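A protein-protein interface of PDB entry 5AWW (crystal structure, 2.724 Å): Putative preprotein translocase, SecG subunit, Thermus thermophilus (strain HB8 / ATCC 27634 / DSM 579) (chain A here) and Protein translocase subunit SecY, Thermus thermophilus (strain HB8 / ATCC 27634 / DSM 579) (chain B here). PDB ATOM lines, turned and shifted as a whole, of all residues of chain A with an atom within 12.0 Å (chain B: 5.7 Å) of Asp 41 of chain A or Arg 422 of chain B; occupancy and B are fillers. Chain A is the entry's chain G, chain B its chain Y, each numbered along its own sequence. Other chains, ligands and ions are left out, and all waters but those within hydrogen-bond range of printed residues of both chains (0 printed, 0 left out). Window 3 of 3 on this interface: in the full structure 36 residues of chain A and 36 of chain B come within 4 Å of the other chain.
O of Gln 418 of chain B sits close to OD2 of Asp 41 of chain A (3.5 Å). NE2 of Gln 418 of chain B sits at hydrogen-bond distance from O of Gly 38 of chain A, at 2.5 Å. NH2 of Arg 422 of chain B sits at hydrogen-bond distance from O of Asp 41 of chain A. NH2 of Arg 17 of chain B lies within hydrogen-bond range of O of Leu 42 of chain A, at 3.3 Å. The side-chain amide oxygen (OE1) of Gln 418 of chain B sits at hydrogen-bond distance from the backbone NH (N) of Ala 40 of chain A, 2.6 Å away.
The guanidinium group (NH1) of Arg 422 of chain B lies within salt-bridge range of the side-chain carboxylate (OE1) of Glu 13 of chain B, at 3.4 Å.
O of Ser 39 of chain A touches NH2 of Arg 17 of chain B, 3.7 Å away. Ser 39 of chain A touches Gln 418 of chain B (CA to NE2, 3.4 Å). Leu 14 of chain B touches Ala 40 of chain A. CA of Ala 40 of chain A touches NH2 of Arg 17 of chain B, 3.4 Å away.
Printed residues of chain B within 4 Å of Asp 41 of chain A: Gln 418 (3.5 Å) and Arg 422 (3.4 Å). Arg 422 of chain B touches just one residue of chain A: Asp 41. No residue of chain A comes within 4 Å of Ile 11 of chain B. Of chain A, only Gly 38 (2.5 Å), Ser 39 (3.4 Å), Ala 40 (2.6 Å) and Asp 41 (3.5 Å) come within 4 Å of Gln 418 of chain B. No residue of chain A comes within 4 Å of Leu 419 of chain B. No residue of chain A comes within 4 Å of Ser 423 of chain B. No residue of chain A comes within 4 Å of Tyr 424 of chain B. Printed residues of chain B within 4 Å of Gly 38 of chain A: Gln 418. Printed residues of chain A within 4 Å of Leu 14 of chain B: Ala 40 (3.9 Å). Printed residues of chain B within 4 Å of Leu 42 of chain A: Arg 17. Printed residues of chain B within 4 Å of Ser 39 of chain A: Arg 17 and Gln 418. Phe 43 of chain A touches none of the printed residues of chain B. The nearest residue of chain B that does not touch Asp 41 of chain A is Leu 419 of chain B (4.6 Å). The nearest printed residue of chain B that does not touch Ser 39 of chain A is Leu 14 of chain B (7.4 Å).
Of the 11 printed residues of chain B, 4 touch a printed residue of chain A. Hydrophobic or aromatic side chains of chain B that line the printed part of chain A: Leu 14. Of the 11 printed residues of chain A, 5 touch a printed residue of chain B. Hydrophobic or aromatic side chains of chain A within 4 Å of the printed part of chain B: Ala 40. Among the printed residues, 9 pairs touch across the chains.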
ATOM      1  N   MET A  36      -6.024  -2.964 -30.195  1.00  0.00           N
ATOM      2  CA  MET A  36      -4.977  -3.885 -30.621  1.00  0.00           C
ATOM      3  C   MET A  36      -4.465  -4.695 -29.435  1.00  0.00           C
ATOM      4  O   MET A  36      -4.862  -4.460 -28.296  1.00  0.00           O
ATOM      5  CB  MET A  36      -3.821  -3.126 -31.278  1.00  0.00           C
ATOM      6  CG  MET A  36      -3.903  -3.029 -32.793  1.00  0.00           C
ATOM      7  SD  MET A  36      -3.593  -4.610 -33.607  1.00  0.00           S
ATOM      8  CE  MET A  36      -3.646  -4.126 -35.330  1.00  0.00           C
ATOM      9  N   GLY A  37      -3.583  -5.651 -29.709  1.00  0.00           N
ATOM     10  CA  GLY A  37      -2.952  -6.419 -28.653  1.00  0.00           C
ATOM     11  C   GLY A  37      -1.792  -5.649 -28.053  1.00  0.00           C
ATOM     12  O   GLY A  37      -1.368  -5.912 -26.928  1.00  0.00           O
ATOM     13  N   GLY A  38      -1.280  -4.687 -28.817  1.00  0.00           N
ATOM     14  CA  GLY A  38      -0.167  -3.868 -28.377  1.00  0.00           C
ATOM     15  C   GLY A  38       1.156  -4.608 -28.407  1.00  0.00           C
ATOM     16  O   GLY A  38       1.191  -5.839 -28.403  1.00  0.00           O
ATOM     17  N   SER A  39       2.250  -3.855 -28.442  1.00  0.00           N
ATOM     18  CA  SER A  39       3.584  -4.445 -28.410  1.00  0.00           C
ATOM     19  C   SER A  39       3.862  -5.070 -27.046  1.00  0.00           C
ATOM     20  O   SER A  39       4.062  -4.364 -26.056  1.00  0.00           O
ATOM     21  CB  SER A  39       4.641  -3.394 -28.747  1.00  0.00           C
ATOM     22  OG  SER A  39       4.364  -2.168 -28.093  1.00  0.00           O
ATOM     23  N   ALA A  40       3.871  -6.399 -27.003  1.00  0.00           N
ATOM     24  CA  ALA A  40       4.035  -7.131 -25.752  1.00  0.00           C
ATOM     25  C   ALA A  40       5.493  -7.499 -25.486  1.00  0.00           C
ATOM     26  O   ALA A  40       5.778  -8.405 -24.701  1.00  0.00           O
ATOM     27  CB  ALA A  40       3.171  -8.384 -25.761  1.00  0.00           C
ATOM     28  N   ASP A  41       6.411  -6.797 -26.143  1.00  0.00           N
ATOM     29  CA  ASP A  41       7.838  -7.026 -25.941  1.00  0.00           C
ATOM     30  C   ASP A  41       8.364  -6.230 -24.752  1.00  0.00           C
ATOM     31  O   ASP A  41       9.086  -6.764 -23.909  1.00  0.00           O
ATOM     32  CB  ASP A  41       8.626  -6.660 -27.202  1.00  0.00           C
ATOM     33  CG  ASP A  41       8.578  -7.748 -28.254  1.00  0.00           C
ATOM     34  OD1 ASP A  41       7.601  -8.526 -28.263  1.00  0.00           O
ATOM     35  OD2 ASP A  41       9.519  -7.823 -29.073  1.00  0.00           O
ATOM     36  N   LEU A  42       8.004  -4.952 -24.695  1.00  0.00           N
ATOM     37  CA  LEU A  42       8.414  -4.093 -23.591  1.00  0.00           C
ATOM     38  C   LEU A  42       7.747  -4.533 -22.292  1.00  0.00           C
ATOM     39  O   LEU A  42       6.548  -4.812 -22.263  1.00  0.00           O
ATOM     40  CB  LEU A  42       8.083  -2.627 -23.886  1.00  0.00           C
ATOM     41  CG  LEU A  42       6.644  -2.286 -24.281  1.00  0.00           C
ATOM     42  CD1 LEU A  42       6.209  -0.975 -23.646  1.00  0.00           C
ATOM     43  CD2 LEU A  42       6.523  -2.208 -25.790  1.00  0.00           C
ATOM     44  N   PHE A  43       8.533  -4.599 -21.223  1.00  0.00           N
ATOM     45  CA  PHE A  43       8.018  -4.999 -19.921  1.00  0.00           C
ATOM     46  C   PHE A  43       7.052  -3.954 -19.374  1.00  0.00           C
ATOM     47  O   PHE A  43       6.105  -4.290 -18.659  1.00  0.00           O
ATOM     48  CB  PHE A  43       9.169  -5.227 -18.936  1.00  0.00           C
ATOM     49  CG  PHE A  43       8.720  -5.543 -17.536  1.00  0.00           C
ATOM     50  CD1 PHE A  43       8.222  -6.796 -17.220  1.00  0.00           C
ATOM     51  CD2 PHE A  43       8.804  -4.589 -16.535  1.00  0.00           C
ATOM     52  CE1 PHE A  43       7.811  -7.090 -15.931  1.00  0.00           C
ATOM     53  CE2 PHE A  43       8.395  -4.877 -15.246  1.00  0.00           C
ATOM     54  CZ  PHE A  43       7.898  -6.128 -14.944  1.00  0.00           C
ATOM     55  N   SER A  44       7.298  -2.693 -19.728  1.00  0.00           N
ATOM     56  CA  SER A  44       6.487  -1.570 -19.264  1.00  0.00           C
ATOM     57  C   SER A  44       6.379  -1.569 -17.743  1.00  0.00           C
ATOM     58  O   SER A  44       7.388  -1.462 -17.045  1.00  0.00           O
ATOM     59  CB  SER A  44       5.093  -1.610 -19.898  1.00  0.00           C
ATOM     60  OG  SER A  44       4.295  -0.527 -19.449  1.00  0.00           O
ATOM     61  N   ALA A  45       5.152  -1.699 -17.246  1.00  0.00           N
ATOM     62  CA  ALA A  45       4.877  -1.772 -15.811  1.00  0.00           C
ATOM     63  C   ALA A  45       5.511  -0.621 -15.036  1.00  0.00           C
ATOM     64  O   ALA A  45       6.060  -0.820 -13.951  1.00  0.00           O
ATOM     65  CB  ALA A  45       5.349  -3.108 -15.252  1.00  0.00           C
ATOM     66  N   ARG A  46       5.435   0.581 -15.599  1.00  0.00           N
ATOM     67  CA  ARG A  46       5.907   1.782 -14.920  1.00  0.00           C
ATOM     68  C   ARG A  46       4.985   2.080 -13.740  1.00  0.00           C
ATOM     69  O   ARG A  46       3.965   1.413 -13.562  1.00  0.00           O
ATOM     70  CB  ARG A  46       5.955   2.966 -15.892  1.00  0.00           C
ATOM     71  CG  ARG A  46       7.145   3.908 -15.717  1.00  0.00           C
ATOM     72  CD  ARG A  46       6.797   5.121 -14.862  1.00  0.00           C
ATOM     73  NE  ARG A  46       5.622   5.832 -15.361  1.00  0.00           N
ATOM     74  CZ  ARG A  46       5.671   6.907 -16.142  1.00  0.00           C
ATOM     75  NH1 ARG A  46       4.549   7.486 -16.545  1.00  0.00           N
ATOM     76  NH2 ARG A  46       6.841   7.406 -16.517  1.00  0.00           N
ATOM     77  N   ILE B  11       8.444 -18.376 -23.141  1.00  0.00           N
ATOM     78  CA  ILE B  11       9.112 -17.102 -22.878  1.00  0.00           C
ATOM     79  C   ILE B  11       8.533 -16.396 -21.652  1.00  0.00           C
ATOM     80  O   ILE B  11       7.329 -16.144 -21.592  1.00  0.00           O
ATOM     81  CB  ILE B  11       9.007 -16.162 -24.096  1.00  0.00           C
ATOM     82  CG1 ILE B  11       9.617 -16.823 -25.333  1.00  0.00           C
ATOM     83  CG2 ILE B  11       9.682 -14.833 -23.813  1.00  0.00           C
ATOM     84  CD1 ILE B  11       9.459 -16.009 -26.598  1.00  0.00           C
ATOM     85  N   GLU B  13       8.427 -13.310 -20.392  1.00  0.00           N
ATOM     86  CA  GLU B  13       7.615 -12.109 -20.561  1.00  0.00           C
ATOM     87  C   GLU B  13       6.214 -12.463 -21.049  1.00  0.00           C
ATOM     88  O   GLU B  13       5.205 -12.052 -20.458  1.00  0.00           O
ATOM     89  CB  GLU B  13       8.282 -11.138 -21.540  1.00  0.00           C
ATOM     90  CG  GLU B  13       9.597 -10.541 -21.052  1.00  0.00           C
ATOM     91  CD  GLU B  13      10.788 -11.456 -21.276  1.00  0.00           C
ATOM     92  OE1 GLU B  13      10.586 -12.626 -21.662  1.00  0.00           O
ATOM     93  OE2 GLU B  13      11.934 -11.002 -21.069  1.00  0.00           O
ATOM     94  N   LEU B  14       6.162 -13.235 -22.129  1.00  0.00           N
ATOM     95  CA  LEU B  14       4.895 -13.636 -22.718  1.00  0.00           C
ATOM     96  C   LEU B  14       4.098 -14.540 -21.786  1.00  0.00           C
ATOM     97  O   LEU B  14       2.871 -14.503 -21.786  1.00  0.00           O
ATOM     98  CB  LEU B  14       5.124 -14.337 -24.056  1.00  0.00           C
ATOM     99  CG  LEU B  14       5.758 -13.472 -25.148  1.00  0.00           C
ATOM    100  CD1 LEU B  14       5.795 -14.217 -26.474  1.00  0.00           C
ATOM    101  CD2 LEU B  14       5.013 -12.152 -25.287  1.00  0.00           C
ATOM    102  N   ARG B  17       2.489 -12.324 -19.370  1.00  0.00           N
ATOM    103  CA  ARG B  17       1.311 -11.784 -20.044  1.00  0.00           C
ATOM    104  C   ARG B  17       0.141 -12.769 -20.014  1.00  0.00           C
ATOM    105  O   ARG B  17      -1.012 -12.393 -19.756  1.00  0.00           O
ATOM    106  CB  ARG B  17       1.648 -11.429 -21.490  1.00  0.00           C
ATOM    107  CG  ARG B  17       2.649 -10.298 -21.649  1.00  0.00           C
ATOM    108  CD  ARG B  17       1.936  -8.977 -21.876  1.00  0.00           C
ATOM    109  NE  ARG B  17       2.865  -7.887 -22.157  1.00  0.00           N
ATOM    110  CZ  ARG B  17       2.490  -6.654 -22.479  1.00  0.00           C
ATOM    111  NH1 ARG B  17       1.201  -6.354 -22.564  1.00  0.00           N
ATOM    112  NH2 ARG B  17       3.400  -5.722 -22.717  1.00  0.00           N
ATOM    113  N   GLN B 418       5.238 -10.248 -33.213  1.00  0.00           N
ATOM    114  CA  GLN B 418       6.068  -9.498 -32.280  1.00  0.00           C
ATOM    115  C   GLN B 418       7.315 -10.282 -31.869  1.00  0.00           C
ATOM    116  O   GLN B 418       8.412  -9.717 -31.793  1.00  0.00           O
ATOM    117  CB  GLN B 418       5.255  -9.098 -31.049  1.00  0.00           C
ATOM    118  CG  GLN B 418       4.192  -8.050 -31.344  1.00  0.00           C
ATOM    119  CD  GLN B 418       3.391  -7.664 -30.119  1.00  0.00           C
ATOM    120  OE1 GLN B 418       3.742  -8.021 -28.994  1.00  0.00           O
ATOM    121  NE2 GLN B 418       2.302  -6.933 -30.331  1.00  0.00           N
ATOM    122  N   LEU B 419       7.159 -11.579 -31.613  1.00  0.00           N
ATOM    123  CA  LEU B 419       8.311 -12.403 -31.262  1.00  0.00           C
ATOM    124  C   LEU B 419       9.264 -12.516 -32.451  1.00  0.00           C
ATOM    125  O   LEU B 419      10.474 -12.684 -32.276  1.00  0.00           O
ATOM    126  CB  LEU B 419       7.875 -13.792 -30.779  1.00  0.00           C
ATOM    127  CG  LEU B 419       7.127 -14.754 -31.707  1.00  0.00           C
ATOM    128  CD1 LEU B 419       8.074 -15.595 -32.558  1.00  0.00           C
ATOM    129  CD2 LEU B 419       6.215 -15.647 -30.886  1.00  0.00           C
ATOM    130  N   MET B 420       8.714 -12.422 -33.660  1.00  0.00           N
ATOM    131  CA  MET B 420       9.541 -12.374 -34.861  1.00  0.00           C
ATOM    132  C   MET B 420      10.440 -11.142 -34.839  1.00  0.00           C
ATOM    133  O   MET B 420      11.621 -11.216 -35.180  1.00  0.00           O
ATOM    134  CB  MET B 420       8.676 -12.374 -36.122  1.00  0.00           C
ATOM    135  CG  MET B 420       9.374 -11.804 -37.348  1.00  0.00           C
ATOM    136  SD  MET B 420       8.546 -12.204 -38.899  1.00  0.00           S
ATOM    137  CE  MET B 420       8.930 -13.947 -39.042  1.00  0.00           C
ATOM    138  N   LEU B 421       9.875 -10.013 -34.425  1.00  0.00           N
ATOM    139  CA  LEU B 421      10.629  -8.769 -34.325  1.00  0.00           C
ATOM    140  C   LEU B 421      11.636  -8.823 -33.180  1.00  0.00           C
ATOM    141  O   LEU B 421      12.687  -8.182 -33.240  1.00  0.00           O
ATOM    142  CB  LEU B 421       9.685  -7.578 -34.148  1.00  0.00           C
ATOM    143  CG  LEU B 421       8.835  -7.212 -35.367  1.00  0.00           C
ATOM    144  CD1 LEU B 421       7.945  -6.014 -35.070  1.00  0.00           C
ATOM    145  CD2 LEU B 421       9.721  -6.939 -36.574  1.00  0.00           C
ATOM    146  N   ARG B 422      11.315  -9.584 -32.136  1.00  0.00           N
ATOM    147  CA  ARG B 422      12.257  -9.787 -31.037  1.00  0.00           C
ATOM    148  C   ARG B 422      13.466 -10.602 -31.492  1.00  0.00           C
ATOM    149  O   ARG B 422      14.606 -10.272 -31.162  1.00  0.00           O
ATOM    150  CB  ARG B 422      11.579 -10.477 -29.849  1.00  0.00           C
ATOM    151  CG  ARG B 422      12.559 -11.177 -28.913  1.00  0.00           C
ATOM    152  CD  ARG B 422      11.936 -11.524 -27.571  1.00  0.00           C
ATOM    153  NE  ARG B 422      11.723 -10.341 -26.743  1.00  0.00           N
ATOM    154  CZ  ARG B 422      11.497 -10.374 -25.434  1.00  0.00           C
ATOM    155  NH1 ARG B 422      11.458 -11.535 -24.794  1.00  0.00           N
ATOM    156  NH2 ARG B 422      11.314  -9.245 -24.761  1.00  0.00           N
ATOM    157  N   SER B 423      13.211 -11.663 -32.253  1.00  0.00           N
ATOM    158  CA  SER B 423      14.281 -12.528 -32.744  1.00  0.00           C
ATOM    159  C   SER B 423      15.242 -11.776 -33.665  1.00  0.00           C
ATOM    160  O   SER B 423      16.438 -12.065 -33.696  1.00  0.00           O
ATOM    161  CB  SER B 423      13.697 -13.739 -33.478  1.00  0.00           C
ATOM    162  OG  SER B 423      12.956 -13.338 -34.617  1.00  0.00           O
ATOM    163  N   TYR B 424      14.710 -10.811 -34.409  1.00  0.00           N
ATOM    164  CA  TYR B 424      15.520 -10.005 -35.315  1.00  0.00           C
ATOM    165  C   TYR B 424      15.556  -8.547 -34.872  1.00  0.00           C
ATOM    166  O   TYR B 424      16.627  -7.971 -34.682  1.00  0.00           O
ATOM    167  CB  TYR B 424      14.988 -10.107 -36.746  1.00  0.00           C
